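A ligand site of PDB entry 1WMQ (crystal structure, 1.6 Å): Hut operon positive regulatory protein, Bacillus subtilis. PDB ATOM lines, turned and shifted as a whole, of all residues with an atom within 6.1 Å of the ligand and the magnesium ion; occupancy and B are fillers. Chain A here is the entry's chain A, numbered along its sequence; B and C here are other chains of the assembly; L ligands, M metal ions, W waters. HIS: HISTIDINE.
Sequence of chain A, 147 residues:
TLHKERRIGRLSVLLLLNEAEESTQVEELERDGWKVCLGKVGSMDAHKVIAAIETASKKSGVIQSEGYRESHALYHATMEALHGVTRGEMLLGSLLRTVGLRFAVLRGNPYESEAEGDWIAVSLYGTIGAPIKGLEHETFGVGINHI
NE2 of the ligand lies close to N of Ala 130.
OXT of the ligand lies within salt-bridge range of NH1 of Arg 97 (2.8 Å).
The side-chain hydroxyl (OH) of Tyr 68 of chain B lies within hydrogen-bond range of a nitrogen (ND1) of the ligand.
The guanidinium group (NH2) of Arg 87 lies within salt-bridge range of an oxygen (OXT) of the ligand (2.9 Å).
The side-chain hydroxyl of Tyr 75 of chain B lies within hydrogen-bond range of the backbone carbonyl oxygen of Leu 95 (2.6 Å).
The backbone carbonyl oxygen (O) of Val 85 is in hydrogen-bond range of the guanidinium group (NH2) of Arg 87 (2.8 Å).
O of His 137 sits at hydrogen-bond distance from N of Ile 128 (2.9 Å).
The backbone NH (N) of Thr 98 sits at hydrogen-bond distance from the backbone carbonyl oxygen (O) of Gly 129, at 2.9 Å.
The guanidinium group (NH2) of Arg 97 is in hydrogen-bond range of the backbone carbonyl oxygen (O) of Thr 86, 3.1 Å away.
N of Ala 130 is in hydrogen-bond range of O of Leu 135 (2.9 Å).
OE1 of Glu 80 of chain C lies within salt-bridge range of NH1 of Arg 87 (2.9 Å).
Ile 128 touches the ligand (CD1 to OXT, 3.6 Å).
Gly 129 touches the ligand (CA to CG, 3.5 Å).
Tyr 75 of chain B touches the ligand (CD1 to NE2, 3.4 Å).
Hydrophobic or aromatic side chains within 4 Å of the ligand: Ile 128, Ala 130, His 137, Tyr 68 of chain B, Tyr 75 of chain B and His 76 of chain B.
Of the 23 residues printed, 9 come within 4 Å of the ligand.
Within 4 Å of the magnesium ion: His 137, His 72 of chain B and His 76 of chain B.
The nearest printed residue that does not touch the magnesium ion is Arg 87 (4.2 Å).
O of the ligand binds the magnesium ion, at 2.1 Å.
The magnesium ion is bound by water W2 (2.2 Å).
NE2 of His 72 of chain B is bound to the magnesium ion (2.3 Å).
NE2 of His 76 of chain B binds the magnesium ion (2.3 Å).
The magnesium ion is bound by NE2 of His 137, at 2.3 Å.
Water W2 bridges the side-chain carboxylate (OE1) of Glu 80 of chain C (2.7 Å) and the backbone carbonyl oxygen (O) of Ile 144 of chain C (2.7 Å).
Water W1 lies within hydrogen-bond range of the backbone carbonyl oxygen (O) of Leu 96 (2.7 Å) and a nitrogen (NE2) of the ligand (2.8 Å).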
ATOM      1  N   VAL A  85     -14.126  29.831 -10.249  1.00  0.00           N
ATOM      2  CA  VAL A  85     -13.435  29.705  -8.976  1.00  0.00           C
ATOM      3  C   VAL A  85     -12.489  28.518  -8.927  1.00  0.00           C
ATOM      4  O   VAL A  85     -11.362  28.655  -8.457  1.00  0.00           O
ATOM      5  CB  VAL A  85     -14.457  29.598  -7.812  1.00  0.00           C
ATOM      6  CG1 VAL A  85     -13.755  29.202  -6.520  1.00  0.00           C
ATOM      7  CG2 VAL A  85     -15.159  30.942  -7.629  1.00  0.00           C
ATOM      8  N   THR A  86     -12.927  27.362  -9.436  1.00  0.00           N
ATOM      9  CA  THR A  86     -12.129  26.148  -9.413  1.00  0.00           C
ATOM     10  C   THR A  86     -11.222  25.903 -10.608  1.00  0.00           C
ATOM     11  O   THR A  86     -10.235  25.172 -10.507  1.00  0.00           O
ATOM     12  CB  THR A  86     -13.008  24.905  -9.194  1.00  0.00           C
ATOM     13  OG1 THR A  86     -14.019  24.846 -10.203  1.00  0.00           O
ATOM     14  CG2 THR A  86     -13.672  24.976  -7.810  1.00  0.00           C
ATOM     15  N   ARG A  87     -11.574  26.485 -11.751  1.00  0.00           N
ATOM     16  CA  ARG A  87     -10.777  26.376 -12.963  1.00  0.00           C
ATOM     17  C   ARG A  87     -10.297  24.987 -13.416  1.00  0.00           C
ATOM     18  O   ARG A  87      -9.091  24.753 -13.566  1.00  0.00           O
ATOM     19  CB  ARG A  87      -9.572  27.327 -12.848  1.00  0.00           C
ATOM     20  CG  ARG A  87      -9.943  28.807 -12.900  1.00  0.00           C
ATOM     21  CD  ARG A  87      -9.033  29.655 -12.013  1.00  0.00           C
ATOM     22  NE  ARG A  87      -9.234  29.294 -10.601  1.00  0.00           N
ATOM     23  CZ  ARG A  87      -8.276  28.854  -9.793  1.00  0.00           C
ATOM     24  NH1 ARG A  87      -7.031  28.725 -10.212  1.00  0.00           N
ATOM     25  NH2 ARG A  87      -8.586  28.496  -8.551  1.00  0.00           N
ATOM     26  N   LEU A  95      -8.624  18.306  -3.119  1.00  0.00           N
ATOM     27  CA  LEU A  95      -7.410  18.711  -3.818  1.00  0.00           C
ATOM     28  C   LEU A  95      -6.593  19.612  -2.907  1.00  0.00           C
ATOM     29  O   LEU A  95      -5.805  20.447  -3.357  1.00  0.00           O
ATOM     30  CB  LEU A  95      -7.752  19.447  -5.126  1.00  0.00           C
ATOM     31  CG  LEU A  95      -8.412  18.622  -6.228  1.00  0.00           C
ATOM     32  CD1 LEU A  95      -8.551  19.492  -7.473  1.00  0.00           C
ATOM     33  CD2 LEU A  95      -7.582  17.381  -6.523  1.00  0.00           C
ATOM     34  N   LEU A  96      -6.794  19.436  -1.610  1.00  0.00           N
ATOM     35  CA  LEU A  96      -6.070  20.186  -0.595  1.00  0.00           C
ATOM     36  C   LEU A  96      -6.108  21.713  -0.740  1.00  0.00           C
ATOM     37  O   LEU A  96      -5.084  22.389  -0.653  1.00  0.00           O
ATOM     38  CB  LEU A  96      -4.628  19.679  -0.522  1.00  0.00           C
ATOM     39  CG  LEU A  96      -3.867  19.936   0.785  1.00  0.00           C
ATOM     40  CD1 LEU A  96      -4.637  19.334   1.954  1.00  0.00           C
ATOM     41  CD2 LEU A  96      -2.484  19.320   0.684  1.00  0.00           C
ATOM     42  N   ARG A  97      -7.296  22.241  -0.996  1.00  0.00           N
ATOM     43  CA  ARG A  97      -7.454  23.684  -1.096  1.00  0.00           C
ATOM     44  C   ARG A  97      -8.749  24.129  -0.436  1.00  0.00           C
ATOM     45  O   ARG A  97      -9.707  23.356  -0.291  1.00  0.00           O
ATOM     46  CB  ARG A  97      -7.363  24.176  -2.557  1.00  0.00           C
ATOM     47  CG  ARG A  97      -8.399  23.662  -3.510  1.00  0.00           C
ATOM     48  CD  ARG A  97      -8.187  24.279  -4.910  1.00  0.00           C
ATOM     49  NE  ARG A  97      -9.136  23.729  -5.864  1.00  0.00           N
ATOM     50  CZ  ARG A  97      -9.162  24.003  -7.160  1.00  0.00           C
ATOM     51  NH1 ARG A  97      -8.280  24.847  -7.691  1.00  0.00           N
ATOM     52  NH2 ARG A  97     -10.073  23.419  -7.930  1.00  0.00           N
ATOM     53  N   THR A  98      -8.754  25.383  -0.026  1.00  0.00           N
ATOM     54  CA  THR A  98      -9.889  25.959   0.680  1.00  0.00           C
ATOM     55  C   THR A  98     -10.257  27.282   0.039  1.00  0.00           C
ATOM     56  O   THR A  98      -9.412  27.931  -0.594  1.00  0.00           O
ATOM     57  CB  THR A  98      -9.495  26.203   2.159  1.00  0.00           C
ATOM     58  OG1 THR A  98     -10.534  26.932   2.827  1.00  0.00           O
ATOM     59  CG2 THR A  98      -8.194  27.005   2.244  1.00  0.00           C
ATOM     60  N   ILE A 128      -8.574  31.560  -2.660  1.00  0.00           N
ATOM     61  CA  ILE A 128      -8.507  30.107  -2.721  1.00  0.00           C
ATOM     62  C   ILE A 128      -7.030  29.813  -2.457  1.00  0.00           C
ATOM     63  O   ILE A 128      -6.160  30.555  -2.893  1.00  0.00           O
ATOM     64  CB  ILE A 128      -8.967  29.587  -4.119  1.00  0.00           C
ATOM     65  CG1 ILE A 128      -9.062  28.066  -4.115  1.00  0.00           C
ATOM     66  CG2 ILE A 128      -8.024  30.097  -5.209  1.00  0.00           C
ATOM     67  CD1 ILE A 128      -9.733  27.474  -5.360  1.00  0.00           C
ATOM     68  N   GLY A 129      -6.749  28.756  -1.708  1.00  0.00           N
ATOM     69  CA  GLY A 129      -5.359  28.459  -1.435  1.00  0.00           C
ATOM     70  C   GLY A 129      -5.184  27.202  -0.631  1.00  0.00           C
ATOM     71  O   GLY A 129      -6.122  26.437  -0.451  1.00  0.00           O
ATOM     72  N   ALA A 130      -3.968  26.978  -0.159  1.00  0.00           N
ATOM     73  CA  ALA A 130      -3.672  25.830   0.659  1.00  0.00           C
ATOM     74  C   ALA A 130      -4.323  26.145   1.999  1.00  0.00           C
ATOM     75  O   ALA A 130      -4.600  27.297   2.305  1.00  0.00           O
ATOM     76  CB  ALA A 130      -2.178  25.667   0.826  1.00  0.00           C
ATOM     77  N   PRO A 131      -4.581  25.122   2.817  1.00  0.00           N
ATOM     78  CA  PRO A 131      -5.202  25.314   4.126  1.00  0.00           C
ATOM     79  C   PRO A 131      -4.195  25.942   5.088  1.00  0.00           C
ATOM     80  O   PRO A 131      -3.815  25.344   6.094  1.00  0.00           O
ATOM     81  CB  PRO A 131      -5.582  23.891   4.553  1.00  0.00           C
ATOM     82  CG  PRO A 131      -5.460  23.064   3.295  1.00  0.00           C
ATOM     83  CD  PRO A 131      -4.311  23.688   2.577  1.00  0.00           C
ATOM     84  N   LEU A 135      -1.233  31.534   2.333  1.00  0.00           N
ATOM     85  CA  LEU A 135      -0.851  30.768   1.146  1.00  0.00           C
ATOM     86  C   LEU A 135      -2.084  30.687   0.260  1.00  0.00           C
ATOM     87  O   LEU A 135      -2.716  29.631   0.122  1.00  0.00           O
ATOM     88  CB  LEU A 135      -0.372  29.375   1.539  1.00  0.00           C
ATOM     89  CG  LEU A 135       0.788  29.306   2.541  1.00  0.00           C
ATOM     90  CD1 LEU A 135       1.247  27.868   2.699  1.00  0.00           C
ATOM     91  CD2 LEU A 135       1.944  30.164   2.058  1.00  0.00           C
ATOM     92  N   GLU A 136      -2.419  31.815  -0.349  1.00  0.00           N
ATOM     93  CA  GLU A 136      -3.619  31.931  -1.164  1.00  0.00           C
ATOM     94  C   GLU A 136      -3.540  33.093  -2.142  1.00  0.00           C
ATOM     95  O   GLU A 136      -2.677  33.958  -2.020  1.00  0.00           O
ATOM     96  CB  GLU A 136      -4.809  32.185  -0.231  1.00  0.00           C
ATOM     97  CG  GLU A 136      -4.642  33.520   0.526  1.00  0.00           C
ATOM     98  CD  GLU A 136      -5.425  33.584   1.831  1.00  0.00           C
ATOM     99  OE1 GLU A 136      -5.345  32.615   2.601  1.00  0.00           O
ATOM    100  OE2 GLU A 136      -6.097  34.612   2.074  1.00  0.00           O
ATOM    101  N   HIS A 137      -4.450  33.088  -3.113  1.00  0.00           N
ATOM    102  CA  HIS A 137      -4.574  34.183  -4.051  1.00  0.00           C
ATOM    103  C   HIS A 137      -6.065  34.360  -4.340  1.00  0.00           C
ATOM    104  O   HIS A 137      -6.884  33.536  -3.931  1.00  0.00           O
ATOM    105  CB  HIS A 137      -3.740  33.978  -5.338  1.00  0.00           C
ATOM    106  CG  HIS A 137      -4.114  32.782  -6.164  1.00  0.00           C
ATOM    107  ND1 HIS A 137      -5.338  32.654  -6.780  1.00  0.00           N
ATOM    108  CD2 HIS A 137      -3.384  31.708  -6.539  1.00  0.00           C
ATOM    109  CE1 HIS A 137      -5.346  31.554  -7.513  1.00  0.00           C
ATOM    110  NE2 HIS A 137      -4.169  30.968  -7.380  1.00  0.00           N
ATOM    111  N   TYR B  68       4.518  31.960  -0.320  1.00  0.00           N
ATOM    112  CA  TYR B  68       3.534  31.243  -1.126  1.00  0.00           C
ATOM    113  C   TYR B  68       4.051  30.928  -2.514  1.00  0.00           C
ATOM    114  O   TYR B  68       3.816  29.848  -3.040  1.00  0.00           O
ATOM    115  CB  TYR B  68       2.257  32.077  -1.232  1.00  0.00           C
ATOM    116  CG  TYR B  68       1.126  31.404  -1.981  1.00  0.00           C
ATOM    117  CD1 TYR B  68       0.771  30.085  -1.731  1.00  0.00           C
ATOM    118  CD2 TYR B  68       0.359  32.129  -2.894  1.00  0.00           C
ATOM    119  CE1 TYR B  68      -0.324  29.489  -2.359  1.00  0.00           C
ATOM    120  CE2 TYR B  68      -0.746  31.552  -3.529  1.00  0.00           C
ATOM    121  CZ  TYR B  68      -1.082  30.230  -3.256  1.00  0.00           C
ATOM    122  OH  TYR B  68      -2.186  29.674  -3.863  1.00  0.00           O
ATOM    123  N   SER B  71       5.338  27.503  -3.251  1.00  0.00           N
ATOM    124  CA  SER B  71       4.331  26.489  -2.951  1.00  0.00           C
ATOM    125  C   SER B  71       3.286  26.524  -4.053  1.00  0.00           C
ATOM    126  O   SER B  71       2.734  25.491  -4.457  1.00  0.00           O
ATOM    127  CB  SER B  71       3.662  26.753  -1.607  1.00  0.00           C
ATOM    128  OG  SER B  71       4.574  26.541  -0.540  1.00  0.00           O
ATOM    129  N   HIS B  72       3.008  27.724  -4.561  1.00  0.00           N
ATOM    130  CA  HIS B  72       2.030  27.887  -5.628  1.00  0.00           C
ATOM    131  C   HIS B  72       2.524  27.165  -6.874  1.00  0.00           C
ATOM    132  O   HIS B  72       1.772  26.464  -7.542  1.00  0.00           O
ATOM    133  CB  HIS B  72       1.792  29.374  -5.924  1.00  0.00           C
ATOM    134  CG  HIS B  72       0.732  29.620  -6.947  1.00  0.00           C
ATOM    135  ND1 HIS B  72       1.016  29.922  -8.260  1.00  0.00           N
ATOM    136  CD2 HIS B  72      -0.612  29.603  -6.854  1.00  0.00           C
ATOM    137  CE1 HIS B  72      -0.107  30.077  -8.929  1.00  0.00           C
ATOM    138  NE2 HIS B  72      -1.114  29.897  -8.098  1.00  0.00           N
ATOM    139  N   TYR B  75       2.270  23.372  -6.333  1.00  0.00           N
ATOM    140  CA  TYR B  75       0.889  22.898  -6.343  1.00  0.00           C
ATOM    141  C   TYR B  75       0.401  22.675  -7.765  1.00  0.00           C
ATOM    142  O   TYR B  75      -0.159  21.630  -8.079  1.00  0.00           O
ATOM    143  CB  TYR B  75      -0.046  23.913  -5.665  1.00  0.00           C
ATOM    144  CG  TYR B  75      -1.464  23.423  -5.601  1.00  0.00           C
ATOM    145  CD1 TYR B  75      -1.847  22.471  -4.653  1.00  0.00           C
ATOM    146  CD2 TYR B  75      -2.440  23.890  -6.487  1.00  0.00           C
ATOM    147  CE1 TYR B  75      -3.154  21.997  -4.581  1.00  0.00           C
ATOM    148  CE2 TYR B  75      -3.745  23.422  -6.435  1.00  0.00           C
ATOM    149  CZ  TYR B  75      -4.104  22.486  -5.479  1.00  0.00           C
ATOM    150  OH  TYR B  75      -5.409  22.033  -5.380  1.00  0.00           O
ATOM    151  N   HIS B  76       0.632  23.661  -8.618  1.00  0.00           N
ATOM    152  CA  HIS B  76       0.183  23.544  -9.994  1.00  0.00           C
ATOM    153  C   HIS B  76       0.946  22.499 -10.775  1.00  0.00           C
ATOM    154  O   HIS B  76       0.385  21.853 -11.656  1.00  0.00           O
ATOM    155  CB  HIS B  76       0.236  24.902 -10.668  1.00  0.00           C
ATOM    156  CG  HIS B  76      -0.906  25.788 -10.282  1.00  0.00           C
ATOM    157  ND1 HIS B  76      -2.168  25.640 -10.813  1.00  0.00           N
ATOM    158  CD2 HIS B  76      -0.995  26.779  -9.361  1.00  0.00           C
ATOM    159  CE1 HIS B  76      -2.984  26.515 -10.255  1.00  0.00           C
ATOM    160  NE2 HIS B  76      -2.298  27.212  -9.365  1.00  0.00           N
ATOM    161  N   GLU C  80      -6.495  30.004 -17.205  1.00  0.00           N
ATOM    162  CA  GLU C  80      -7.367  30.041 -16.034  1.00  0.00           C
ATOM    163  C   GLU C  80      -8.509  31.033 -16.194  1.00  0.00           C
ATOM    164  O   GLU C  80      -9.636  30.750 -15.795  1.00  0.00           O
ATOM    165  CB  GLU C  80      -6.537  30.306 -14.768  1.00  0.00           C
ATOM    166  CG  GLU C  80      -5.686  29.074 -14.398  1.00  0.00           C
ATOM    167  CD  GLU C  80      -5.035  29.151 -13.030  1.00  0.00           C
ATOM    168  OE1 GLU C  80      -5.432  30.004 -12.217  1.00  0.00           O
ATOM    169  OE2 GLU C  80      -4.128  28.329 -12.756  1.00  0.00           O
ATOM    170  N   TRP C 119       3.329  38.909  -9.559  1.00  0.00           N
ATOM    171  CA  TRP C 119       2.270  37.989  -9.930  1.00  0.00           C
ATOM    172  C   TRP C 119       1.543  38.651 -11.076  1.00  0.00           C
ATOM    173  O   TRP C 119       1.693  39.844 -11.314  1.00  0.00           O
ATOM    174  CB  TRP C 119       1.316  37.753  -8.753  1.00  0.00           C
ATOM    175  CG  TRP C 119       1.928  36.921  -7.670  1.00  0.00           C
ATOM    176  CD1 TRP C 119       3.026  37.232  -6.923  1.00  0.00           C
ATOM    177  CD2 TRP C 119       1.521  35.608  -7.267  1.00  0.00           C
ATOM    178  NE1 TRP C 119       3.326  36.194  -6.073  1.00  0.00           N
ATOM    179  CE2 TRP C 119       2.426  35.190  -6.260  1.00  0.00           C
ATOM    180  CE3 TRP C 119       0.483  34.757  -7.657  1.00  0.00           C
ATOM    181  CZ2 TRP C 119       2.320  33.942  -5.645  1.00  0.00           C
ATOM    182  CZ3 TRP C 119       0.384  33.514  -7.040  1.00  0.00           C
ATOM    183  CH2 TRP C 119       1.289  33.123  -6.046  1.00  0.00           C
ATOM    184  N   ILE C 144      -4.994  34.001 -12.227  1.00  0.00           N
ATOM    185  CA  ILE C 144      -3.895  34.614 -11.489  1.00  0.00           C
ATOM    186  C   ILE C 144      -2.714  33.644 -11.423  1.00  0.00           C
ATOM    187  O   ILE C 144      -2.897  32.456 -11.208  1.00  0.00           O
ATOM    188  CB  ILE C 144      -4.362  34.983 -10.059  1.00  0.00           C
ATOM    189  CG1 ILE C 144      -5.327  36.183 -10.116  1.00  0.00           C
ATOM    190  CG2 ILE C 144      -3.154  35.347  -9.179  1.00  0.00           C
ATOM    191  CD1 ILE C 144      -6.042  36.485  -8.819  1.00  0.00           C
ATOM    192  N   ASN C 145      -1.505  34.161 -11.630  1.00  0.00           N
ATOM    193  CA  ASN C 145      -0.320  33.304 -11.615  1.00  0.00           C
ATOM    194  C   ASN C 145       0.910  34.063 -11.133  1.00  0.00           C
ATOM    195  O   ASN C 145       0.938  35.293 -11.176  1.00  0.00           O
ATOM    196  CB  ASN C 145      -0.076  32.758 -13.029  1.00  0.00           C
ATOM    197  CG  ASN C 145       0.713  31.453 -13.022  1.00  0.00           C
ATOM    198  OD1 ASN C 145       0.889  30.812 -11.980  1.00  0.00           O
ATOM    199  ND2 ASN C 145       1.155  31.044 -14.205  1.00  0.00           N
HETATM  200  CA  HIS L   1      -4.342  26.942  -6.246  1.00  0.00           C
HETATM  201  C   HIS L   1      -5.443  27.417  -7.188  1.00  0.00           C
HETATM  202  O   HIS L   1      -5.150  28.166  -8.132  1.00  0.00           O
HETATM  203  CB  HIS L   1      -4.810  26.968  -4.799  1.00  0.00           C
HETATM  204  CG  HIS L   1      -3.816  26.388  -3.848  1.00  0.00           C
HETATM  205  ND1 HIS L   1      -2.649  27.031  -3.512  1.00  0.00           N
HETATM  206  CD2 HIS L   1      -3.770  25.177  -3.246  1.00  0.00           C
HETATM  207  CE1 HIS L   1      -1.920  26.245  -2.747  1.00  0.00           C
HETATM  208  NE2 HIS L   1      -2.574  25.110  -2.564  1.00  0.00           N
HETATM  209  OXT HIS L   1      -6.601  27.015  -6.993  1.00  0.00           O
HETATM  210 MG    MG M   1      -3.246  29.064  -8.355  1.00  0.00          MG
HETATM  211  O   HOH W   1      -2.431  22.890  -0.803  1.00  0.00           O
HETATM  212  O   HOH W   2      -3.538  29.969 -10.342  1.00  0.00           O
